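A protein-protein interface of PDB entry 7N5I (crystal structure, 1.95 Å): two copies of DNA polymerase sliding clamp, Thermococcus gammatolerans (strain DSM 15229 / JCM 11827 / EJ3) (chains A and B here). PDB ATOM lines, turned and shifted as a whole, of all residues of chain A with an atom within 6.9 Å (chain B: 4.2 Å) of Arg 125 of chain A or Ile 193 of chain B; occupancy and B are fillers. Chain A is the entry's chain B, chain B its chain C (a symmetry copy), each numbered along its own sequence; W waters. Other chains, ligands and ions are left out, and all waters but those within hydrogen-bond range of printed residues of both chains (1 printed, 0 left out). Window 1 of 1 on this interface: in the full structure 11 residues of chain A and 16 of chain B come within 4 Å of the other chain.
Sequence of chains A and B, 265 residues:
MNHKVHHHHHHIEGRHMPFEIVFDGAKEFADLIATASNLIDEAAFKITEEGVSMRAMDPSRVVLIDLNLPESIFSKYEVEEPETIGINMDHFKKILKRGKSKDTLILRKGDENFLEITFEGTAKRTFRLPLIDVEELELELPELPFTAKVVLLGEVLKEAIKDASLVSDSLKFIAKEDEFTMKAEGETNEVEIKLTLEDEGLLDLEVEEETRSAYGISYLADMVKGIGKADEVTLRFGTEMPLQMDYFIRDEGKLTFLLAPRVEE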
ATOM      1  N   ALA A  26      32.157  37.736  18.323  1.00  0.00           N
ATOM      2  CA  ALA A  26      30.911  37.517  19.061  1.00  0.00           C
ATOM      3  C   ALA A  26      30.941  38.224  20.403  1.00  0.00           C
ATOM      4  O   ALA A  26      29.920  38.744  20.868  1.00  0.00           O
ATOM      5  CB  ALA A  26      30.662  36.020  19.262  1.00  0.00           C
ATOM      6  N   ILE A  95      23.128  33.761  26.570  1.00  0.00           N
ATOM      7  CA  ILE A  95      23.668  33.012  25.438  1.00  0.00           C
ATOM      8  C   ILE A  95      24.842  33.758  24.814  1.00  0.00           C
ATOM      9  O   ILE A  95      25.913  33.182  24.586  1.00  0.00           O
ATOM     10  CB  ILE A  95      22.559  32.743  24.408  1.00  0.00           C
ATOM     11  CG1 ILE A  95      21.461  31.846  25.015  1.00  0.00           C
ATOM     12  CG2 ILE A  95      23.145  32.132  23.127  1.00  0.00           C
ATOM     13  CD1 ILE A  95      20.216  31.716  24.136  1.00  0.00           C
ATOM     14  N   LYS A  97      26.827  35.753  26.071  1.00  0.00           N
ATOM     15  CA  LYS A  97      27.992  35.703  26.951  1.00  0.00           C
ATOM     16  C   LYS A  97      28.837  34.461  26.712  1.00  0.00           C
ATOM     17  O   LYS A  97      30.011  34.444  27.095  1.00  0.00           O
ATOM     18  CB  LYS A  97      27.575  35.753  28.428  1.00  0.00           C
ATOM     19  CG  LYS A  97      27.350  37.181  28.942  1.00  0.00           C
ATOM     20  CD  LYS A  97      28.144  38.174  28.099  1.00  0.00           C
ATOM     21  CE  LYS A  97      28.283  39.540  28.755  1.00  0.00           C
ATOM     22  NZ  LYS A  97      29.009  40.464  27.829  1.00  0.00           N
ATOM     23  N   ARG A  98      28.281  33.438  26.069  1.00  0.00           N
ATOM     24  CA  ARG A  98      29.077  32.264  25.728  1.00  0.00           C
ATOM     25  C   ARG A  98      29.989  32.485  24.522  1.00  0.00           C
ATOM     26  O   ARG A  98      30.874  31.659  24.286  1.00  0.00           O
ATOM     27  CB  ARG A  98      28.166  31.052  25.458  1.00  0.00           C
ATOM     28  CG  ARG A  98      27.024  30.794  26.492  1.00  0.00           C
ATOM     29  CD  ARG A  98      27.535  30.538  27.916  1.00  0.00           C
ATOM     30  NE  ARG A  98      28.944  30.170  27.971  1.00  0.00           N
ATOM     31  CZ  ARG A  98      29.827  30.775  28.759  1.00  0.00           C
ATOM     32  NH1 ARG A  98      29.439  31.759  29.564  1.00  0.00           N
ATOM     33  NH2 ARG A  98      31.091  30.406  28.733  1.00  0.00           N
ATOM     34  N   GLY A  99      29.814  33.568  23.766  1.00  0.00           N
ATOM     35  CA  GLY A  99      30.638  33.768  22.587  1.00  0.00           C
ATOM     36  C   GLY A  99      32.044  34.202  22.965  1.00  0.00           C
ATOM     37  O   GLY A  99      32.255  34.934  23.930  1.00  0.00           O
ATOM     38  N   LYS A 100      33.019  33.744  22.190  1.00  0.00           N
ATOM     39  CA  LYS A 100      34.405  34.125  22.418  1.00  0.00           C
ATOM     40  C   LYS A 100      34.800  35.287  21.512  1.00  0.00           C
ATOM     41  O   LYS A 100      34.133  35.593  20.522  1.00  0.00           O
ATOM     42  CB  LYS A 100      35.328  32.927  22.199  1.00  0.00           C
ATOM     43  CG  LYS A 100      34.849  31.667  22.904  1.00  0.00           C
ATOM     44  CD  LYS A 100      34.616  31.918  24.393  1.00  0.00           C
ATOM     45  CE  LYS A 100      33.996  30.694  25.072  1.00  0.00           C
ATOM     46  NZ  LYS A 100      33.941  30.802  26.568  1.00  0.00           N
ATOM     47  N   ASP A 103      35.177  34.348  17.998  1.00  0.00           N
ATOM     48  CA  ASP A 103      34.056  33.675  17.340  1.00  0.00           C
ATOM     49  C   ASP A 103      33.410  34.577  16.300  1.00  0.00           C
ATOM     50  O   ASP A 103      33.305  35.792  16.477  1.00  0.00           O
ATOM     51  CB  ASP A 103      32.976  33.252  18.357  1.00  0.00           C
ATOM     52  CG  ASP A 103      33.365  32.022  19.141  1.00  0.00           C
ATOM     53  OD1 ASP A 103      34.178  31.212  18.629  1.00  0.00           O
ATOM     54  OD2 ASP A 103      32.854  31.854  20.268  1.00  0.00           O
ATOM     55  N   ILE A 117      21.256  31.139  17.211  1.00  0.00           N
ATOM     56  CA  ILE A 117      22.449  31.900  17.561  1.00  0.00           C
ATOM     57  C   ILE A 117      23.622  30.946  17.462  1.00  0.00           C
ATOM     58  O   ILE A 117      23.739  30.012  18.272  1.00  0.00           O
ATOM     59  CB  ILE A 117      22.358  32.507  18.971  1.00  0.00           C
ATOM     60  CG1 ILE A 117      21.145  33.440  19.088  1.00  0.00           C
ATOM     61  CG2 ILE A 117      23.662  33.241  19.323  1.00  0.00           C
ATOM     62  CD1 ILE A 117      20.838  33.835  20.531  1.00  0.00           C
ATOM     63  N   THR A 118      24.502  31.174  16.488  1.00  0.00           N
ATOM     64  CA  THR A 118      25.625  30.282  16.265  1.00  0.00           C
ATOM     65  C   THR A 118      26.937  31.009  16.518  1.00  0.00           C
ATOM     66  O   THR A 118      27.120  32.151  16.077  1.00  0.00           O
ATOM     67  CB  THR A 118      25.579  29.727  14.841  1.00  0.00           C
ATOM     68  OG1 THR A 118      24.313  29.083  14.640  1.00  0.00           O
ATOM     69  CG2 THR A 118      26.703  28.726  14.617  1.00  0.00           C
ATOM     70  N   PHE A 119      27.842  30.349  17.239  1.00  0.00           N
ATOM     71  CA  PHE A 119      29.220  30.791  17.377  1.00  0.00           C
ATOM     72  C   PHE A 119      30.107  29.860  16.555  1.00  0.00           C
ATOM     73  O   PHE A 119      30.086  28.638  16.757  1.00  0.00           O
ATOM     74  CB  PHE A 119      29.647  30.790  18.836  1.00  0.00           C
ATOM     75  CG  PHE A 119      28.707  31.533  19.751  1.00  0.00           C
ATOM     76  CD1 PHE A 119      28.519  32.908  19.627  1.00  0.00           C
ATOM     77  CD2 PHE A 119      28.037  30.856  20.767  1.00  0.00           C
ATOM     78  CE1 PHE A 119      27.656  33.599  20.501  1.00  0.00           C
ATOM     79  CE2 PHE A 119      27.187  31.541  21.640  1.00  0.00           C
ATOM     80  CZ  PHE A 119      26.993  32.908  21.498  1.00  0.00           C
ATOM     81  N   GLU A 120      30.877  30.429  15.632  1.00  0.00           N
ATOM     82  CA  GLU A 120      31.777  29.658  14.777  1.00  0.00           C
ATOM     83  C   GLU A 120      33.204  30.061  15.108  1.00  0.00           C
ATOM     84  O   GLU A 120      33.582  31.227  14.937  1.00  0.00           O
ATOM     85  CB  GLU A 120      31.450  29.883  13.307  1.00  0.00           C
ATOM     86  CG  GLU A 120      30.104  29.311  12.930  1.00  0.00           C
ATOM     87  CD  GLU A 120      29.928  29.184  11.434  1.00  0.00           C
ATOM     88  OE1 GLU A 120      30.781  29.720  10.695  1.00  0.00           O
ATOM     89  OE2 GLU A 120      28.944  28.538  11.004  1.00  0.00           O
ATOM     90  N   GLY A 121      33.968  29.110  15.636  1.00  0.00           N
ATOM     91  CA  GLY A 121      35.335  29.336  16.060  1.00  0.00           C
ATOM     92  C   GLY A 121      36.125  28.044  16.003  1.00  0.00           C
ATOM     93  O   GLY A 121      36.239  27.434  14.938  1.00  0.00           O
ATOM     94  N   THR A 122      36.661  27.606  17.141  1.00  0.00           N
ATOM     95  CA  THR A 122      37.286  26.293  17.185  1.00  0.00           C
ATOM     96  C   THR A 122      36.263  25.182  17.031  1.00  0.00           C
ATOM     97  O   THR A 122      36.634  24.050  16.701  1.00  0.00           O
ATOM     98  CB  THR A 122      38.043  26.117  18.492  1.00  0.00           C
ATOM     99  OG1 THR A 122      37.163  26.425  19.579  1.00  0.00           O
ATOM    100  CG2 THR A 122      39.256  27.055  18.536  1.00  0.00           C
ATOM    101  N   ALA A 123      34.990  25.483  17.275  1.00  0.00           N
ATOM    102  CA  ALA A 123      33.900  24.562  17.028  1.00  0.00           C
ATOM    103  C   ALA A 123      32.706  25.375  16.559  1.00  0.00           C
ATOM    104  O   ALA A 123      32.751  26.610  16.507  1.00  0.00           O
ATOM    105  CB  ALA A 123      33.570  23.741  18.284  1.00  0.00           C
ATOM    106  N   LYS A 124      31.628  24.677  16.233  1.00  0.00           N
ATOM    107  CA  LYS A 124      30.366  25.295  15.862  1.00  0.00           C
ATOM    108  C   LYS A 124      29.367  25.061  16.991  1.00  0.00           C
ATOM    109  O   LYS A 124      29.026  23.913  17.293  1.00  0.00           O
ATOM    110  CB  LYS A 124      29.856  24.719  14.544  1.00  0.00           C
ATOM    111  CG  LYS A 124      28.625  25.395  13.993  1.00  0.00           C
ATOM    112  CD  LYS A 124      27.987  24.529  12.910  1.00  0.00           C
ATOM    113  CE  LYS A 124      26.971  25.301  12.091  1.00  0.00           C
ATOM    114  NZ  LYS A 124      25.919  24.390  11.549  1.00  0.00           N
ATOM    115  N   ARG A 125      28.910  26.140  17.618  1.00  0.00           N
ATOM    116  CA  ARG A 125      28.013  26.061  18.768  1.00  0.00           C
ATOM    117  C   ARG A 125      26.732  26.813  18.440  1.00  0.00           C
ATOM    118  O   ARG A 125      26.766  28.021  18.179  1.00  0.00           O
ATOM    119  CB  ARG A 125      28.687  26.632  20.011  1.00  0.00           C
ATOM    120  CG  ARG A 125      29.993  25.926  20.314  1.00  0.00           C
ATOM    121  CD  ARG A 125      30.620  26.479  21.558  1.00  0.00           C
ATOM    122  NE  ARG A 125      31.162  27.806  21.322  1.00  0.00           N
ATOM    123  CZ  ARG A 125      31.021  28.832  22.155  1.00  0.00           C
ATOM    124  NH1 ARG A 125      30.342  28.699  23.291  1.00  0.00           N
ATOM    125  NH2 ARG A 125      31.562  29.997  21.851  1.00  0.00           N
ATOM    126  N   THR A 126      25.612  26.096  18.441  1.00  0.00           N
ATOM    127  CA  THR A 126      24.335  26.636  17.996  1.00  0.00           C
ATOM    128  C   THR A 126      23.335  26.562  19.138  1.00  0.00           C
ATOM    129  O   THR A 126      23.043  25.471  19.643  1.00  0.00           O
ATOM    130  CB  THR A 126      23.807  25.872  16.781  1.00  0.00           C
ATOM    131  OG1 THR A 126      24.760  25.942  15.720  1.00  0.00           O
ATOM    132  CG2 THR A 126      22.501  26.474  16.304  1.00  0.00           C
ATOM    133  N   PHE A 127      22.825  27.718  19.547  1.00  0.00           N
ATOM    134  CA  PHE A 127      21.760  27.820  20.530  1.00  0.00           C
ATOM    135  C   PHE A 127      20.456  28.179  19.835  1.00  0.00           C
ATOM    136  O   PHE A 127      20.438  28.905  18.835  1.00  0.00           O
ATOM    137  CB  PHE A 127      22.049  28.896  21.587  1.00  0.00           C
ATOM    138  CG  PHE A 127      23.288  28.654  22.409  1.00  0.00           C
ATOM    139  CD1 PHE A 127      24.547  28.843  21.867  1.00  0.00           C
ATOM    140  CD2 PHE A 127      23.179  28.305  23.748  1.00  0.00           C
ATOM    141  CE1 PHE A 127      25.696  28.654  22.645  1.00  0.00           C
ATOM    142  CE2 PHE A 127      24.309  28.115  24.525  1.00  0.00           C
ATOM    143  CZ  PHE A 127      25.569  28.284  23.968  1.00  0.00           C
ATOM    144  N   GLU B 159      33.770  24.471  27.296  1.00  0.00           N
ATOM    145  CA  GLU B 159      32.728  25.403  26.883  1.00  0.00           C
ATOM    146  C   GLU B 159      31.444  24.666  26.526  1.00  0.00           C
ATOM    147  O   GLU B 159      30.344  25.144  26.826  1.00  0.00           O
ATOM    148  CB  GLU B 159      33.216  26.257  25.711  1.00  0.00           C
ATOM    149  CG  GLU B 159      32.341  27.463  25.408  1.00  0.00           C
ATOM    150  CD  GLU B 159      32.048  28.317  26.638  1.00  0.00           C
ATOM    151  OE1 GLU B 159      30.862  28.631  26.874  1.00  0.00           O
ATOM    152  OE2 GLU B 159      33.000  28.671  27.376  1.00  0.00           O
ATOM    153  N   ALA B 160      31.556  23.490  25.907  1.00  0.00           N
ATOM    154  CA  ALA B 160      30.350  22.739  25.567  1.00  0.00           C
ATOM    155  C   ALA B 160      29.583  22.336  26.824  1.00  0.00           C
ATOM    156  O   ALA B 160      28.347  22.333  26.836  1.00  0.00           O
ATOM    157  CB  ALA B 160      30.718  21.507  24.738  1.00  0.00           C
ATOM    158  N   ASP B 163      27.953  25.509  28.134  1.00  0.00           N
ATOM    159  CA  ASP B 163      26.840  25.793  27.225  1.00  0.00           C
ATOM    160  C   ASP B 163      25.632  24.906  27.507  1.00  0.00           C
ATOM    161  O   ASP B 163      24.482  25.377  27.545  1.00  0.00           O
ATOM    162  CB  ASP B 163      27.278  25.568  25.768  1.00  0.00           C
ATOM    163  CG  ASP B 163      28.330  26.560  25.278  1.00  0.00           C
ATOM    164  OD1 ASP B 163      28.607  27.567  25.957  1.00  0.00           O
ATOM    165  OD2 ASP B 163      28.883  26.310  24.188  1.00  0.00           O
ATOM    166  N   PHE B 180      31.354  14.894  15.386  1.00  0.00           N
ATOM    167  CA  PHE B 180      31.106  14.641  16.800  1.00  0.00           C
ATOM    168  C   PHE B 180      30.235  15.781  17.300  1.00  0.00           C
ATOM    169  O   PHE B 180      30.588  16.953  17.119  1.00  0.00           O
ATOM    170  CB  PHE B 180      32.413  14.552  17.597  1.00  0.00           C
ATOM    171  CG  PHE B 180      32.220  14.506  19.094  1.00  0.00           C
ATOM    172  CD1 PHE B 180      31.538  13.456  19.697  1.00  0.00           C
ATOM    173  CD2 PHE B 180      32.733  15.506  19.899  1.00  0.00           C
ATOM    174  CE1 PHE B 180      31.362  13.412  21.072  1.00  0.00           C
ATOM    175  CE2 PHE B 180      32.564  15.471  21.276  1.00  0.00           C
ATOM    176  CZ  PHE B 180      31.878  14.421  21.862  1.00  0.00           C
ATOM    177  N   THR B 181      29.088  15.442  17.889  1.00  0.00           N
ATOM    178  CA  THR B 181      28.105  16.419  18.342  1.00  0.00           C
ATOM    179  C   THR B 181      27.810  16.183  19.816  1.00  0.00           C
ATOM    180  O   THR B 181      27.652  15.034  20.243  1.00  0.00           O
ATOM    181  CB  THR B 181      26.816  16.320  17.517  1.00  0.00           C
ATOM    182  OG1 THR B 181      27.114  16.575  16.141  1.00  0.00           O
ATOM    183  CG2 THR B 181      25.787  17.346  17.989  1.00  0.00           C
ATOM    184  N   MET B 182      27.789  17.263  20.592  1.00  0.00           N
ATOM    185  CA  MET B 182      27.295  17.250  21.961  1.00  0.00           C
ATOM    186  C   MET B 182      26.040  18.108  21.959  1.00  0.00           C
ATOM    187  O   MET B 182      26.082  19.263  21.524  1.00  0.00           O
ATOM    188  CB  MET B 182      28.344  17.772  22.943  1.00  0.00           C
ATOM    189  CG  MET B 182      29.606  16.912  22.994  1.00  0.00           C
ATOM    190  SD  MET B 182      30.967  17.593  23.964  1.00  0.00           S
ATOM    191  CE  MET B 182      31.634  18.712  22.719  1.00  0.00           C
ATOM    192  N   GLU B 192      23.611  22.739  20.531  1.00  0.00           N
ATOM    193  CA  GLU B 192      24.403  21.702  19.891  1.00  0.00           C
ATOM    194  C   GLU B 192      25.797  22.261  19.673  1.00  0.00           C
ATOM    195  O   GLU B 192      25.946  23.386  19.185  1.00  0.00           O
ATOM    196  CB  GLU B 192      23.790  21.281  18.553  1.00  0.00           C
ATOM    197  CG  GLU B 192      22.357  20.806  18.644  1.00  0.00           C
ATOM    198  CD  GLU B 192      21.780  20.482  17.281  1.00  0.00           C
ATOM    199  OE1 GLU B 192      22.523  20.621  16.284  1.00  0.00           O
ATOM    200  OE2 GLU B 192      20.593  20.092  17.203  1.00  0.00           O
ATOM    201  N   ILE B 193      26.810  21.500  20.069  1.00  0.00           N
ATOM    202  CA  ILE B 193      28.202  21.817  19.764  1.00  0.00           C
ATOM    203  C   ILE B 193      28.666  20.759  18.780  1.00  0.00           C
ATOM    204  O   ILE B 193      28.647  19.564  19.098  1.00  0.00           O
ATOM    205  CB  ILE B 193      29.084  21.840  21.020  1.00  0.00           C
ATOM    206  CG1 ILE B 193      28.532  22.853  22.042  1.00  0.00           C
ATOM    207  CG2 ILE B 193      30.558  22.147  20.658  1.00  0.00           C
ATOM    208  CD1 ILE B 193      27.560  22.234  23.055  1.00  0.00           C
ATOM    209  N   LYS B 194      29.027  21.180  17.602  1.00  0.00           N
ATOM    210  CA  LYS B 194      29.440  20.303  16.540  1.00  0.00           C
ATOM    211  C   LYS B 194      30.882  20.460  16.111  1.00  0.00           C
ATOM    212  O   LYS B 194      31.337  21.529  15.955  1.00  0.00           O
ATOM    213  CB  LYS B 194      28.555  20.579  15.393  1.00  0.00           C
ATOM    214  CG  LYS B 194      28.761  19.711  14.197  1.00  0.00           C
ATOM    215  CD  LYS B 194      27.445  19.596  13.485  1.00  0.00           C
ATOM    216  CE  LYS B 194      27.600  19.394  12.001  1.00  0.00           C
ATOM    217  NZ  LYS B 194      28.599  18.378  11.668  1.00  0.00           N
HETATM  218  O   HOH W   1      26.158  23.581  15.966  1.00  0.00           O
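Hydrophobic or aromatic side chains of chain A that line the printed part of chain B: Ala 123 and Phe 127. Hydrophobic or aromatic side chains of chain B within 4 Å of the printed part of chain A: Ile 193. Among the printed residues, Asp or Glu carboxylates within 4 Å of a Lys or Arg side-chain nitrogen of the other chain: Arg 98 of chain A with Glu 159 of chain B, Arg 98 of chain A with Asp 163 of chain B, Lys 100 of chain A with Glu 159 of chain B, Arg 125 of chain A with Glu 159 of chain B and Arg 125 of chain A with Asp 163 of chain B.
Of the printed residues of chain B, Arg 125 of chain A touches Glu 159 (3.2 Å), Asp 163 (2.9 Å), Glu 192 (3.4 Å) and Ile 193 (3.8 Å). Ile 193 of chain B touches just these residues of chain A: Lys 124 and Arg 125. Printed residues of chain B within 4 Å of Ala 123 of chain A: Lys 194. Of the printed residues of chain B, Arg 98 of chain A touches Glu 159 and Asp 163. Of the printed residues of chain B, Phe 127 of chain A touches Asp 163 (3.5 Å). The nearest printed residue of chain B that does not touch Arg 125 of chain A is Lys 194 of chain B (5.0 Å). The nearest printed residue of chain A that does not touch Asp 163 of chain B is Phe 119 of chain A (5.8 Å).
Water W1 lies within hydrogen-bond range of OG1 of Thr 126 of chain A, O of Lys 124 of chain A and O of Glu 192 of chain B.
No position is printed for both chains. Of the 13 pairs that touch across the chains among the printed residues, none has its exchanged pair printed and touching as well.
The guanidinium group of Arg 98 of chain A is in salt-bridge range of the side-chain carboxylate of Glu 159 of chain B (2.6 Å). The side-chain carboxylate (OD1) of Asp 163 of chain B lies within salt-bridge range of the guanidinium group (NE) of Arg 98 of chain A (3.3 Å). The side-chain amino group of Lys 100 of chain A is in salt-bridge range of the side-chain carboxylate of Glu 159 of chain B, 2.5 Å away. The backbone NH (N) of Lys 194 of chain B lies within hydrogen-bond range of the backbone carbonyl oxygen (O) of Lys 124 of chain A (2.8 Å). The side-chain carboxylate (OE1) of Glu 159 of chain B lies within salt-bridge range of the guanidinium group (NH1) of Arg 125 of chain A (3.6 Å). NH1 of Arg 125 of chain A is in salt-bridge range of OD2 of Asp 163 of chain B, at 2.9 Å. O of Glu 192 of chain B lies within hydrogen-bond range of N of Thr 126 of chain A (2.8 Å).
Among the printed residues, merely in contact across the chains: Ala 123 of chain A with Lys 194 of chain B (3.9 Å), Lys 124 of chain A with Glu 192 of chain B (3.7 Å), Lys 124 of chain A with Ile 193 of chain B (3.3 Å), Arg 125 of chain A with Glu 192 of chain B (3.4 Å), Arg 125 of chain A with Ile 193 of chain B (3.8 Å) and Phe 127 of chain A with Asp 163 of chain B (3.5 Å).
The backbone NH (N) of Lys 100 of chain A lies within hydrogen-bond range of the side-chain carboxylate (OD2) of Asp 103 of chain A (2.7 Å). NH2 of Arg 125 of chain A is in salt-bridge range of OD2 of Asp 103 of chain A (2.8 Å). The backbone carbonyl oxygen of Ile 117 of chain A sits at hydrogen-bond distance from the backbone NH of Phe 127 of chain A (2.8 Å). The side-chain hydroxyl (OG1) of Thr 118 of chain A is in hydrogen-bond range of the side-chain hydroxyl (OG1) of Thr 126 of chain A, 3.4 Å away. N of Phe 119 of chain A is in hydrogen-bond range of O of Arg 125 of chain A, at 2.7 Å. O of Met 182 of chain B is in hydrogen-bond range of N of Ile 193 of chain B, 2.8 Å away.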
